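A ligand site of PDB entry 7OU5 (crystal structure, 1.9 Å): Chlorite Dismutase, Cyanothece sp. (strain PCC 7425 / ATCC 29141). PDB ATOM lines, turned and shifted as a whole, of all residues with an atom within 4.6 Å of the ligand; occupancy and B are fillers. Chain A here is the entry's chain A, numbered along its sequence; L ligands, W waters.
N1 of the ligand lies close to NH2 of Arg 133, at 3.4 Å. Residues that only touch the ligand: Phe 151, Phe 147, Thr 121, Ile 65, Gly 124, Leu 164, Phe 114, Met 168, Trp 174, Leu 76, Leu 165, Trp 102, Leu 135, Ile 96, Leu 128, Thr 149, Val 131, Ile 94, Glu 180 and Leu 125.
Water W4 lies within hydrogen-bond range of OH of Tyr 67, O4 of the ligand and NE1 of Trp 102. Water W1 lies within hydrogen-bond range of O2 of the ligand (2.6 Å) and O of Asn 64 (2.8 Å).
The backbone NH of Ile 94 lies within hydrogen-bond range of the backbone carbonyl oxygen of Thr 149, 2.8 Å away. NE1 of Trp 174 is in hydrogen-bond range of OE2 of Glu 180. The backbone carbonyl oxygen (O) of Ile 96 is in hydrogen-bond range of the backbone NH (N) of Phe 147 (2.9 Å). The guanidinium group (NH2) of Arg 169 lies within salt-bridge range of the side-chain carboxylate (OE1) of Glu 180 (2.5 Å). O of Asn 64 sits at hydrogen-bond distance from NE of Arg 66 (3.1 Å). The backbone NH of His 120 sits at hydrogen-bond distance from the backbone carbonyl oxygen of Phe 114, 3.2 Å away. ND1 of His 120 is in hydrogen-bond range of OE2 of Glu 173, 2.9 Å away. OE1 of Glu 173 is in salt-bridge range of NZ of Lys 98 (2.8 Å).
The backbone NH (N) of Tyr 67 sits at hydrogen-bond distance from an oxygen (O1) of the ligand (2.9 Å). A ring nitrogen (NE2) of His 120 binds an iron atom (FE1) of the ligand (2.1 Å). An oxygen (O1) of the ligand sits at hydrogen-bond distance from the backbone NH (N) of Ala 68 (3.0 Å). The side-chain amino group (NZ) of Lys 98 is in salt-bridge range of an oxygen (O4) of the ligand (2.9 Å). The backbone NH (N) of Arg 66 sits at hydrogen-bond distance from an oxygen (O2) of the ligand (2.7 Å).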
ATOM      1  N   ASN A  64     -15.172   5.165  17.550  1.00  0.00           N
ATOM      2  CA  ASN A  64     -16.038   5.310  16.405  1.00  0.00           C
ATOM      3  C   ASN A  64     -16.116   6.763  15.924  1.00  0.00           C
ATOM      4  O   ASN A  64     -15.836   7.712  16.655  1.00  0.00           O
ATOM      5  CB  ASN A  64     -17.445   4.808  16.731  1.00  0.00           C
ATOM      6  CG  ASN A  64     -18.088   5.577  17.891  1.00  0.00           C
ATOM      7  OD1 ASN A  64     -17.791   5.340  19.058  1.00  0.00           O
ATOM      8  ND2 ASN A  64     -18.997   6.465  17.572  1.00  0.00           N
ATOM      9  N   ILE A  65     -16.575   6.909  14.691  1.00  0.00           N
ATOM     10  CA  ILE A  65     -16.759   8.224  14.086  1.00  0.00           C
ATOM     11  C   ILE A  65     -17.827   8.984  14.858  1.00  0.00           C
ATOM     12  O   ILE A  65     -18.877   8.437  15.224  1.00  0.00           O
ATOM     13  CB  ILE A  65     -17.124   8.033  12.600  1.00  0.00           C
ATOM     14  CG1 ILE A  65     -15.884   7.610  11.806  1.00  0.00           C
ATOM     15  CG2 ILE A  65     -17.783   9.269  12.033  1.00  0.00           C
ATOM     16  CD1 ILE A  65     -14.784   8.691  11.709  1.00  0.00           C
ATOM     17  N   ARG A  66     -17.563  10.262  15.090  1.00  0.00           N
ATOM     18  CA  ARG A  66     -18.468  11.140  15.830  1.00  0.00           C
ATOM     19  C   ARG A  66     -19.168  12.193  14.987  1.00  0.00           C
ATOM     20  O   ARG A  66     -20.238  12.663  15.415  1.00  0.00           O
ATOM     21  CB  ARG A  66     -17.721  11.863  16.957  1.00  0.00           C
ATOM     22  CG  ARG A  66     -16.883  10.910  17.835  1.00  0.00           C
ATOM     23  CD  ARG A  66     -17.777   9.777  18.431  1.00  0.00           C
ATOM     24  NE  ARG A  66     -16.968   8.943  19.303  1.00  0.00           N
ATOM     25  CZ  ARG A  66     -16.713   9.235  20.569  1.00  0.00           C
ATOM     26  NH1 ARG A  66     -17.236  10.317  21.137  1.00  0.00           N
ATOM     27  NH2 ARG A  66     -15.961   8.399  21.303  1.00  0.00           N
ATOM     28  N   TYR A  67     -18.629  12.562  13.804  1.00  0.00           N
ATOM     29  CA  TYR A  67     -19.167  13.670  13.033  1.00  0.00           C
ATOM     30  C   TYR A  67     -19.170  13.394  11.530  1.00  0.00           C
ATOM     31  O   TYR A  67     -20.082  13.845  10.822  1.00  0.00           O
ATOM     32  CB  TYR A  67     -18.325  14.948  13.266  1.00  0.00           C
ATOM     33  CG  TYR A  67     -18.382  15.476  14.686  1.00  0.00           C
ATOM     34  CD1 TYR A  67     -19.533  16.089  15.166  1.00  0.00           C
ATOM     35  CD2 TYR A  67     -17.302  15.347  15.538  1.00  0.00           C
ATOM     36  CE1 TYR A  67     -19.602  16.566  16.465  1.00  0.00           C
ATOM     37  CE2 TYR A  67     -17.356  15.830  16.843  1.00  0.00           C
ATOM     38  CZ  TYR A  67     -18.512  16.435  17.295  1.00  0.00           C
ATOM     39  OH  TYR A  67     -18.583  16.894  18.585  1.00  0.00           O
ATOM     40  N   ALA A  68     -18.167  12.674  11.034  1.00  0.00           N
ATOM     41  CA  ALA A  68     -18.052  12.479   9.584  1.00  0.00           C
ATOM     42  C   ALA A  68     -19.253  11.736   9.027  1.00  0.00           C
ATOM     43  O   ALA A  68     -19.747  10.760   9.607  1.00  0.00           O
ATOM     44  CB  ALA A  68     -16.788  11.671   9.263  1.00  0.00           C
ATOM     45  N   LEU A  76     -12.119  10.478   2.510  1.00  0.00           N
ATOM     46  CA  LEU A  76     -10.959  10.229   3.353  1.00  0.00           C
ATOM     47  C   LEU A  76     -10.341   8.877   3.057  1.00  0.00           C
ATOM     48  O   LEU A  76      -9.113   8.751   2.979  1.00  0.00           O
ATOM     49  CB  LEU A  76     -11.376  10.295   4.828  1.00  0.00           C
ATOM     50  CG  LEU A  76     -11.770  11.691   5.339  1.00  0.00           C
ATOM     51  CD1 LEU A  76     -12.577  11.556   6.596  1.00  0.00           C
ATOM     52  CD2 LEU A  76     -10.538  12.554   5.601  1.00  0.00           C
ATOM     53  N   ILE A  94      -0.210  16.154  19.109  1.00  0.00           N
ATOM     54  CA  ILE A  94      -0.887  17.374  19.530  1.00  0.00           C
ATOM     55  C   ILE A  94      -2.055  17.058  20.459  1.00  0.00           C
ATOM     56  O   ILE A  94      -3.164  16.808  19.970  1.00  0.00           O
ATOM     57  CB  ILE A  94      -1.370  18.186  18.321  1.00  0.00           C
ATOM     58  CG1 ILE A  94      -0.158  18.452  17.370  1.00  0.00           C
ATOM     59  CG2 ILE A  94      -1.992  19.505  18.800  1.00  0.00           C
ATOM     60  CD1 ILE A  94      -0.556  19.182  16.098  1.00  0.00           C
ATOM     61  N   ILE A  96      -5.102  18.039  22.789  1.00  0.00           N
ATOM     62  CA  ILE A  96      -6.044  19.155  22.721  1.00  0.00           C
ATOM     63  C   ILE A  96      -7.126  18.986  23.783  1.00  0.00           C
ATOM     64  O   ILE A  96      -7.632  17.882  23.967  1.00  0.00           O
ATOM     65  CB  ILE A  96      -6.676  19.256  21.331  1.00  0.00           C
ATOM     66  CG1 ILE A  96      -5.661  19.829  20.312  1.00  0.00           C
ATOM     67  CG2 ILE A  96      -7.915  20.151  21.356  1.00  0.00           C
ATOM     68  CD1 ILE A  96      -5.896  19.373  18.917  1.00  0.00           C
ATOM     69  N   LYS A  98     -10.875  20.806  24.842  1.00  0.00           N
ATOM     70  CA  LYS A  98     -11.934  21.743  24.462  1.00  0.00           C
ATOM     71  C   LYS A  98     -12.693  22.207  25.702  1.00  0.00           C
ATOM     72  O   LYS A  98     -12.668  21.562  26.743  1.00  0.00           O
ATOM     73  CB  LYS A  98     -12.857  21.102  23.443  1.00  0.00           C
ATOM     74  CG  LYS A  98     -12.190  20.959  22.060  1.00  0.00           C
ATOM     75  CD  LYS A  98     -13.211  20.564  20.956  1.00  0.00           C
ATOM     76  CE  LYS A  98     -12.485  20.286  19.599  1.00  0.00           C
ATOM     77  NZ  LYS A  98     -13.458  20.092  18.464  1.00  0.00           N
ATOM     78  N   TRP A 102     -18.147  23.842  24.831  1.00  0.00           N
ATOM     79  CA  TRP A 102     -18.201  22.915  23.702  1.00  0.00           C
ATOM     80  C   TRP A 102     -18.987  21.663  24.079  1.00  0.00           C
ATOM     81  O   TRP A 102     -19.915  21.249  23.373  1.00  0.00           O
ATOM     82  CB  TRP A 102     -16.802  22.532  23.258  1.00  0.00           C
ATOM     83  CG  TRP A 102     -16.745  21.430  22.202  1.00  0.00           C
ATOM     84  CD1 TRP A 102     -16.446  20.111  22.399  1.00  0.00           C
ATOM     85  CD2 TRP A 102     -17.005  21.570  20.790  1.00  0.00           C
ATOM     86  NE1 TRP A 102     -16.493  19.426  21.210  1.00  0.00           N
ATOM     87  CE2 TRP A 102     -16.826  20.298  20.201  1.00  0.00           C
ATOM     88  CE3 TRP A 102     -17.339  22.663  19.971  1.00  0.00           C
ATOM     89  CZ2 TRP A 102     -16.993  20.068  18.831  1.00  0.00           C
ATOM     90  CZ3 TRP A 102     -17.491  22.439  18.607  1.00  0.00           C
ATOM     91  CH2 TRP A 102     -17.318  21.158  18.060  1.00  0.00           C
ATOM     92  N   PHE A 114     -18.094  22.159  13.631  1.00  0.00           N
ATOM     93  CA  PHE A 114     -16.964  21.344  13.201  1.00  0.00           C
ATOM     94  C   PHE A 114     -16.771  21.425  11.697  1.00  0.00           C
ATOM     95  O   PHE A 114     -15.645  21.571  11.213  1.00  0.00           O
ATOM     96  CB  PHE A 114     -17.191  19.899  13.635  1.00  0.00           C
ATOM     97  CG  PHE A 114     -16.143  18.934  13.167  1.00  0.00           C
ATOM     98  CD1 PHE A 114     -14.925  18.851  13.821  1.00  0.00           C
ATOM     99  CD2 PHE A 114     -16.386  18.103  12.078  1.00  0.00           C
ATOM    100  CE1 PHE A 114     -13.952  17.939  13.403  1.00  0.00           C
ATOM    101  CE2 PHE A 114     -15.432  17.206  11.656  1.00  0.00           C
ATOM    102  CZ  PHE A 114     -14.200  17.132  12.333  1.00  0.00           C
ATOM    103  N   HIS A 120     -13.509  21.361   8.866  1.00  0.00           N
ATOM    104  CA  HIS A 120     -12.385  20.568   9.366  1.00  0.00           C
ATOM    105  C   HIS A 120     -11.970  19.516   8.362  1.00  0.00           C
ATOM    106  O   HIS A 120     -10.785  19.400   8.027  1.00  0.00           O
ATOM    107  CB  HIS A 120     -12.763  19.903  10.693  1.00  0.00           C
ATOM    108  CG  HIS A 120     -11.621  19.250  11.406  1.00  0.00           C
ATOM    109  ND1 HIS A 120     -11.174  19.689  12.619  1.00  0.00           N
ATOM    110  CD2 HIS A 120     -10.869  18.174  11.083  1.00  0.00           C
ATOM    111  CE1 HIS A 120     -10.168  18.914  13.026  1.00  0.00           C
ATOM    112  NE2 HIS A 120      -9.963  17.981  12.109  1.00  0.00           N
ATOM    113  N   THR A 121     -12.929  18.720   7.891  1.00  0.00           N
ATOM    114  CA  THR A 121     -12.606  17.593   7.017  1.00  0.00           C
ATOM    115  C   THR A 121     -12.207  18.063   5.624  1.00  0.00           C
ATOM    116  O   THR A 121     -11.269  17.531   5.038  1.00  0.00           O
ATOM    117  CB  THR A 121     -13.806  16.619   6.946  1.00  0.00           C
ATOM    118  OG1 THR A 121     -14.098  16.180   8.270  1.00  0.00           O
ATOM    119  CG2 THR A 121     -13.488  15.431   6.082  1.00  0.00           C
ATOM    120  N   GLY A 124      -8.707  19.537   5.880  1.00  0.00           N
ATOM    121  CA  GLY A 124      -7.717  18.492   6.109  1.00  0.00           C
ATOM    122  C   GLY A 124      -7.448  17.658   4.886  1.00  0.00           C
ATOM    123  O   GLY A 124      -6.304  17.257   4.639  1.00  0.00           O
ATOM    124  N   LEU A 125      -8.501  17.383   4.094  1.00  0.00           N
ATOM    125  CA  LEU A 125      -8.323  16.546   2.901  1.00  0.00           C
ATOM    126  C   LEU A 125      -7.351  17.181   1.927  1.00  0.00           C
ATOM    127  O   LEU A 125      -6.752  16.478   1.100  1.00  0.00           O
ATOM    128  CB  LEU A 125      -9.658  16.321   2.198  1.00  0.00           C
ATOM    129  CG  LEU A 125     -10.395  15.028   2.598  1.00  0.00           C
ATOM    130  CD1 LEU A 125     -11.899  15.177   2.387  1.00  0.00           C
ATOM    131  CD2 LEU A 125      -9.860  13.848   1.819  1.00  0.00           C
ATOM    132  N   LEU A 128      -3.890  15.696   2.557  1.00  0.00           N
ATOM    133  CA  LEU A 128      -3.743  14.284   2.237  1.00  0.00           C
ATOM    134  C   LEU A 128      -3.370  14.144   0.767  1.00  0.00           C
ATOM    135  O   LEU A 128      -3.846  14.914  -0.088  1.00  0.00           O
ATOM    136  CB  LEU A 128      -5.039  13.538   2.526  1.00  0.00           C
ATOM    137  CG  LEU A 128      -5.171  13.058   3.980  1.00  0.00           C
ATOM    138  CD1 LEU A 128      -5.011  14.220   4.923  1.00  0.00           C
ATOM    139  CD2 LEU A 128      -6.503  12.377   4.237  1.00  0.00           C
ATOM    140  N   VAL A 131       0.002  13.664   4.670  1.00  0.00           N
ATOM    141  CA  VAL A 131      -0.093  13.576   6.118  1.00  0.00           C
ATOM    142  C   VAL A 131      -0.941  12.381   6.511  1.00  0.00           C
ATOM    143  O   VAL A 131      -2.129  12.318   6.142  1.00  0.00           O
ATOM    144  CB  VAL A 131      -0.666  14.874   6.715  1.00  0.00           C
ATOM    145  CG1 VAL A 131      -0.795  14.781   8.273  1.00  0.00           C
ATOM    146  CG2 VAL A 131       0.207  16.074   6.306  1.00  0.00           C
ATOM    147  N   ARG A 133      -2.573  10.250   9.835  1.00  0.00           N
ATOM    148  CA  ARG A 133      -3.090  10.776  11.087  1.00  0.00           C
ATOM    149  C   ARG A 133      -3.779   9.682  11.867  1.00  0.00           C
ATOM    150  O   ARG A 133      -4.238   8.692  11.312  1.00  0.00           O
ATOM    151  CB  ARG A 133      -4.064  11.938  10.845  1.00  0.00           C
ATOM    152  CG  ARG A 133      -5.231  11.510   9.983  1.00  0.00           C
ATOM    153  CD  ARG A 133      -6.203  12.640   9.805  1.00  0.00           C
ATOM    154  NE  ARG A 133      -7.157  12.636  10.906  1.00  0.00           N
ATOM    155  CZ  ARG A 133      -8.272  11.924  10.896  1.00  0.00           C
ATOM    156  NH1 ARG A 133      -8.625  11.210   9.825  1.00  0.00           N
ATOM    157  NH2 ARG A 133      -9.069  11.942  11.981  1.00  0.00           N
ATOM    158  N   LEU A 135      -6.471   9.698  15.388  1.00  0.00           N
ATOM    159  CA  LEU A 135      -7.222  10.448  16.368  1.00  0.00           C
ATOM    160  C   LEU A 135      -7.536   9.528  17.532  1.00  0.00           C
ATOM    161  O   LEU A 135      -8.100   8.455  17.354  1.00  0.00           O
ATOM    162  CB  LEU A 135      -8.517  11.001  15.761  1.00  0.00           C
ATOM    163  CG  LEU A 135      -9.523  11.589  16.750  1.00  0.00           C
ATOM    164  CD1 LEU A 135      -8.936  12.842  17.374  1.00  0.00           C
ATOM    165  CD2 LEU A 135     -10.833  11.880  16.041  1.00  0.00           C
ATOM    166  N   PHE A 147      -8.358  15.102  23.556  1.00  0.00           N
ATOM    167  CA  PHE A 147      -7.956  14.327  22.404  1.00  0.00           C
ATOM    168  C   PHE A 147      -6.435  14.255  22.320  1.00  0.00           C
ATOM    169  O   PHE A 147      -5.726  15.174  22.770  1.00  0.00           O
ATOM    170  CB  PHE A 147      -8.473  14.921  21.077  1.00  0.00           C
ATOM    171  CG  PHE A 147      -9.915  15.293  21.079  1.00  0.00           C
ATOM    172  CD1 PHE A 147     -10.889  14.334  20.805  1.00  0.00           C
ATOM    173  CD2 PHE A 147     -10.328  16.575  21.350  1.00  0.00           C
ATOM    174  CE1 PHE A 147     -12.224  14.659  20.805  1.00  0.00           C
ATOM    175  CE2 PHE A 147     -11.667  16.912  21.347  1.00  0.00           C
ATOM    176  CZ  PHE A 147     -12.622  15.937  21.077  1.00  0.00           C
ATOM    177  N   THR A 149      -4.022  13.836  19.166  1.00  0.00           N
ATOM    178  CA  THR A 149      -3.959  13.743  17.706  1.00  0.00           C
ATOM    179  C   THR A 149      -2.509  13.526  17.278  1.00  0.00           C
ATOM    180  O   THR A 149      -1.596  14.011  17.912  1.00  0.00           O
ATOM    181  CB  THR A 149      -4.542  14.965  17.012  1.00  0.00           C
ATOM    182  OG1 THR A 149      -3.742  16.125  17.291  1.00  0.00           O
ATOM    183  CG2 THR A 149      -5.966  15.192  17.480  1.00  0.00           C
ATOM    184  N   PHE A 151       0.111  12.955  13.807  1.00  0.00           N
ATOM    185  CA  PHE A 151       0.333  13.200  12.394  1.00  0.00           C
ATOM    186  C   PHE A 151       1.761  12.804  12.060  1.00  0.00           C
ATOM    187  O   PHE A 151       2.667  13.004  12.884  1.00  0.00           O
ATOM    188  CB  PHE A 151       0.091  14.683  12.078  1.00  0.00           C
ATOM    189  CG  PHE A 151      -1.215  15.170  12.581  1.00  0.00           C
ATOM    190  CD1 PHE A 151      -2.378  14.948  11.825  1.00  0.00           C
ATOM    191  CD2 PHE A 151      -1.323  15.788  13.811  1.00  0.00           C
ATOM    192  CE1 PHE A 151      -3.609  15.355  12.288  1.00  0.00           C
ATOM    193  CE2 PHE A 151      -2.555  16.197  14.292  1.00  0.00           C
ATOM    194  CZ  PHE A 151      -3.712  15.971  13.543  1.00  0.00           C
ATOM    195  N   PHE A 161       2.193  21.032   6.342  1.00  0.00           N
ATOM    196  CA  PHE A 161       1.563  20.735   7.629  1.00  0.00           C
ATOM    197  C   PHE A 161       1.551  21.986   8.510  1.00  0.00           C
ATOM    198  O   PHE A 161       0.563  22.270   9.200  1.00  0.00           O
ATOM    199  CB  PHE A 161       2.277  19.597   8.324  1.00  0.00           C
ATOM    200  CG  PHE A 161       1.593  19.157   9.596  1.00  0.00           C
ATOM    201  CD1 PHE A 161       0.436  18.420   9.535  1.00  0.00           C
ATOM    202  CD2 PHE A 161       2.092  19.544  10.834  1.00  0.00           C
ATOM    203  CE1 PHE A 161      -0.236  18.035  10.716  1.00  0.00           C
ATOM    204  CE2 PHE A 161       1.468  19.172  11.999  1.00  0.00           C
ATOM    205  CZ  PHE A 161       0.283  18.403  11.941  1.00  0.00           C
ATOM    206  N   LEU A 164      -1.397  24.039   7.436  1.00  0.00           N
ATOM    207  CA  LEU A 164      -2.641  23.472   7.962  1.00  0.00           C
ATOM    208  C   LEU A 164      -2.877  23.878   9.425  1.00  0.00           C
ATOM    209  O   LEU A 164      -3.981  24.294   9.790  1.00  0.00           O
ATOM    210  CB  LEU A 164      -2.587  21.959   7.799  1.00  0.00           C
ATOM    211  CG  LEU A 164      -3.701  21.135   8.490  1.00  0.00           C
ATOM    212  CD1 LEU A 164      -5.068  21.507   7.974  1.00  0.00           C
ATOM    213  CD2 LEU A 164      -3.395  19.686   8.246  1.00  0.00           C
ATOM    214  N   LEU A 165      -1.840  23.784  10.262  1.00  0.00           N
ATOM    215  CA  LEU A 165      -1.985  24.178  11.658  1.00  0.00           C
ATOM    216  C   LEU A 165      -2.483  25.613  11.779  1.00  0.00           C
ATOM    217  O   LEU A 165      -3.373  25.899  12.575  1.00  0.00           O
ATOM    218  CB  LEU A 165      -0.666  24.026  12.402  1.00  0.00           C
ATOM    219  CG  LEU A 165      -0.195  22.626  12.737  1.00  0.00           C
ATOM    220  CD1 LEU A 165       1.129  22.697  13.484  1.00  0.00           C
ATOM    221  CD2 LEU A 165      -1.233  21.841  13.533  1.00  0.00           C
ATOM    222  N   MET A 168      -6.177  25.897  10.823  1.00  0.00           N
ATOM    223  CA  MET A 168      -7.105  25.299  11.799  1.00  0.00           C
ATOM    224  C   MET A 168      -7.200  26.153  13.048  1.00  0.00           C
ATOM    225  O   MET A 168      -8.292  26.281  13.629  1.00  0.00           O
ATOM    226  CB  MET A 168      -6.602  23.910  12.129  1.00  0.00           C
ATOM    227  CG  MET A 168      -6.560  23.056  10.894  1.00  0.00           C
ATOM    228  SD  MET A 168      -6.703  21.327  11.130  1.00  0.00           S
ATOM    229  CE  MET A 168      -8.123  21.210  12.200  1.00  0.00           C
ATOM    230  N   ARG A 169      -6.080  26.773  13.468  1.00  0.00           N
ATOM    231  CA  ARG A 169      -6.077  27.557  14.695  1.00  0.00           C
ATOM    232  C   ARG A 169      -6.870  28.844  14.539  1.00  0.00           C
ATOM    233  O   ARG A 169      -7.236  29.467  15.556  1.00  0.00           O
ATOM    234  CB  ARG A 169      -4.641  27.850  15.101  1.00  0.00           C
ATOM    235  CG  ARG A 169      -3.860  26.574  15.331  1.00  0.00           C
ATOM    236  CD  ARG A 169      -3.796  26.126  16.759  1.00  0.00           C
ATOM    237  NE  ARG A 169      -3.225  24.771  16.841  1.00  0.00           N
ATOM    238  CZ  ARG A 169      -1.920  24.512  16.762  1.00  0.00           C
ATOM    239  NH1 ARG A 169      -1.037  25.465  16.508  1.00  0.00           N
ATOM    240  NH2 ARG A 169      -1.505  23.270  16.955  1.00  0.00           N
ATOM    241  N   GLU A 173     -13.947  26.463  15.146  1.00  0.00           N
ATOM    242  CA  GLU A 173     -13.811  25.329  16.057  1.00  0.00           C
ATOM    243  C   GLU A 173     -12.750  25.606  17.114  1.00  0.00           C
ATOM    244  O   GLU A 173     -12.926  25.226  18.265  1.00  0.00           O
ATOM    245  CB  GLU A 173     -13.480  24.060  15.261  1.00  0.00           C
ATOM    246  CG  GLU A 173     -13.368  22.785  16.078  1.00  0.00           C
ATOM    247  CD  GLU A 173     -12.667  21.659  15.325  1.00  0.00           C
ATOM    248  OE1 GLU A 173     -12.501  20.547  15.911  1.00  0.00           O
ATOM    249  OE2 GLU A 173     -12.260  21.912  14.165  1.00  0.00           O
ATOM    250  N   TRP A 174     -11.650  26.261  16.745  1.00  0.00           N
ATOM    251  CA  TRP A 174     -10.552  26.476  17.691  1.00  0.00           C
ATOM    252  C   TRP A 174     -10.856  27.532  18.749  1.00  0.00           C
ATOM    253  O   TRP A 174     -10.134  27.618  19.738  1.00  0.00           O
ATOM    254  CB  TRP A 174      -9.236  26.844  16.959  1.00  0.00           C
ATOM    255  CG  TRP A 174      -8.233  25.724  17.131  1.00  0.00           C
ATOM    256  CD1 TRP A 174      -7.144  25.707  17.958  1.00  0.00           C
ATOM    257  CD2 TRP A 174      -8.276  24.436  16.499  1.00  0.00           C
ATOM    258  NE1 TRP A 174      -6.507  24.494  17.874  1.00  0.00           N
ATOM    259  CE2 TRP A 174      -7.192  23.696  16.993  1.00  0.00           C
ATOM    260  CE3 TRP A 174      -9.141  23.847  15.564  1.00  0.00           C
ATOM    261  CZ2 TRP A 174      -6.933  22.400  16.567  1.00  0.00           C
ATOM    262  CZ3 TRP A 174      -8.881  22.562  15.159  1.00  0.00           C
ATOM    263  CH2 TRP A 174      -7.795  21.841  15.662  1.00  0.00           C
ATOM    264  N   GLU A 180      -3.595  23.214  24.485  1.00  0.00           N
ATOM    265  CA  GLU A 180      -3.026  22.609  23.286  1.00  0.00           C
ATOM    266  C   GLU A 180      -1.505  22.669  23.368  1.00  0.00           C
ATOM    267  O   GLU A 180      -0.952  23.720  23.684  1.00  0.00           O
ATOM    268  CB  GLU A 180      -3.491  23.336  22.040  1.00  0.00           C
ATOM    269  CG  GLU A 180      -3.081  22.646  20.762  1.00  0.00           C
ATOM    270  CD  GLU A 180      -3.738  23.251  19.540  1.00  0.00           C
ATOM    271  OE1 GLU A 180      -3.459  22.759  18.418  1.00  0.00           O
ATOM    272  OE2 GLU A 180      -4.486  24.258  19.705  1.00  0.00           O
HETATM  273  C1  LIG L   1     -11.312  15.036  14.255  1.00  0.00           C
HETATM  274  C2  LIG L   1      -9.956  14.826   9.608  1.00  0.00           C
HETATM  275  C3  LIG L   1      -6.038  17.393  10.855  1.00  0.00           C
HETATM  276  C4  LIG L   1      -7.594  17.909  15.394  1.00  0.00           C
HETATM  277  C5  LIG L   1     -11.300  14.773  12.904  1.00  0.00           C
HETATM  278  C6  LIG L   1     -12.338  14.093  12.154  1.00  0.00           C
HETATM  279  C7  LIG L   1     -11.943  14.030  10.883  1.00  0.00           C
HETATM  280  C8  LIG L   1     -10.652  14.688  10.774  1.00  0.00           C
HETATM  281  C9  LIG L   1     -12.692  13.441   9.668  1.00  0.00           C
HETATM  282  C10 LIG L   1     -13.684  13.532  12.694  1.00  0.00           C
HETATM  283  C11 LIG L   1     -13.525  12.131  13.184  1.00  0.00           C
HETATM  284  C12 LIG L   1     -14.930  11.741  13.690  1.00  0.00           C
HETATM  285  O1  LIG L   1     -15.930  11.962  12.928  1.00  0.00           O
HETATM  286  O2  LIG L   1     -15.011  11.249  14.839  1.00  0.00           O
HETATM  287  C13 LIG L   1      -8.729  15.479   9.548  1.00  0.00           C
HETATM  288  C14 LIG L   1      -7.834  15.502   8.422  1.00  0.00           C
HETATM  289  C15 LIG L   1      -6.735  16.170   8.773  1.00  0.00           C
HETATM  290  C16 LIG L   1      -6.914  16.630  10.137  1.00  0.00           C
HETATM  291  C17 LIG L   1      -8.092  14.798   7.080  1.00  0.00           C
HETATM  292  C18 LIG L   1      -5.521  16.417   7.837  1.00  0.00           C
HETATM  293  C19 LIG L   1      -4.291  16.390   8.330  1.00  0.00           C
HETATM  294  C20 LIG L   1      -6.122  17.790  12.161  1.00  0.00           C
HETATM  295  C21 LIG L   1      -5.163  18.614  12.892  1.00  0.00           C
HETATM  296  C22 LIG L   1      -5.571  18.725  14.159  1.00  0.00           C
HETATM  297  C23 LIG L   1      -6.838  17.999  14.264  1.00  0.00           C
HETATM  298  C24 LIG L   1      -3.861  19.178  12.289  1.00  0.00           C
HETATM  299  C25 LIG L   1      -4.986  19.476  15.364  1.00  0.00           C
HETATM  300  C26 LIG L   1      -4.163  20.524  15.230  1.00  0.00           C
HETATM  301  C27 LIG L   1      -8.744  17.146  15.497  1.00  0.00           C
HETATM  302  C28 LIG L   1      -9.570  16.983  16.681  1.00  0.00           C
HETATM  303  C29 LIG L   1     -10.581  16.185  16.365  1.00  0.00           C
HETATM  304  C30 LIG L   1     -10.449  15.839  14.966  1.00  0.00           C
HETATM  305  C31 LIG L   1      -9.252  17.627  18.038  1.00  0.00           C
HETATM  306  C32 LIG L   1     -11.751  15.712  17.314  1.00  0.00           C
HETATM  307  C33 LIG L   1     -12.883  16.706  17.113  1.00  0.00           C
HETATM  308  C34 LIG L   1     -14.012  16.436  18.095  1.00  0.00           C
HETATM  309  O3  LIG L   1     -14.399  15.265  18.270  1.00  0.00           O
HETATM  310  O4  LIG L   1     -14.506  17.419  18.693  1.00  0.00           O
HETATM  311  N1  LIG L   1     -10.290  15.121  12.023  1.00  0.00           N
HETATM  312  N2  LIG L   1      -8.159  16.166  10.569  1.00  0.00           N
HETATM  313  N3  LIG L   1      -7.128  17.457  13.033  1.00  0.00           N
HETATM  314  N4  LIG L   1      -9.295  16.452  14.484  1.00  0.00           N
HETATM  315 FE1  LIG L   1      -8.727  16.353  12.539  1.00  0.00          FE
HETATM  316  O   HOH W   1     -13.669   9.409  16.165  1.00  0.00           O
HETATM  317  O   HOH W   2     -16.125  14.081  20.166  1.00  0.00           O
HETATM  318  O   HOH W   3     -14.016  13.174  16.762  1.00  0.00           O
HETATM  319  O   HOH W   4     -16.580  16.737  20.037  1.00  0.00           O
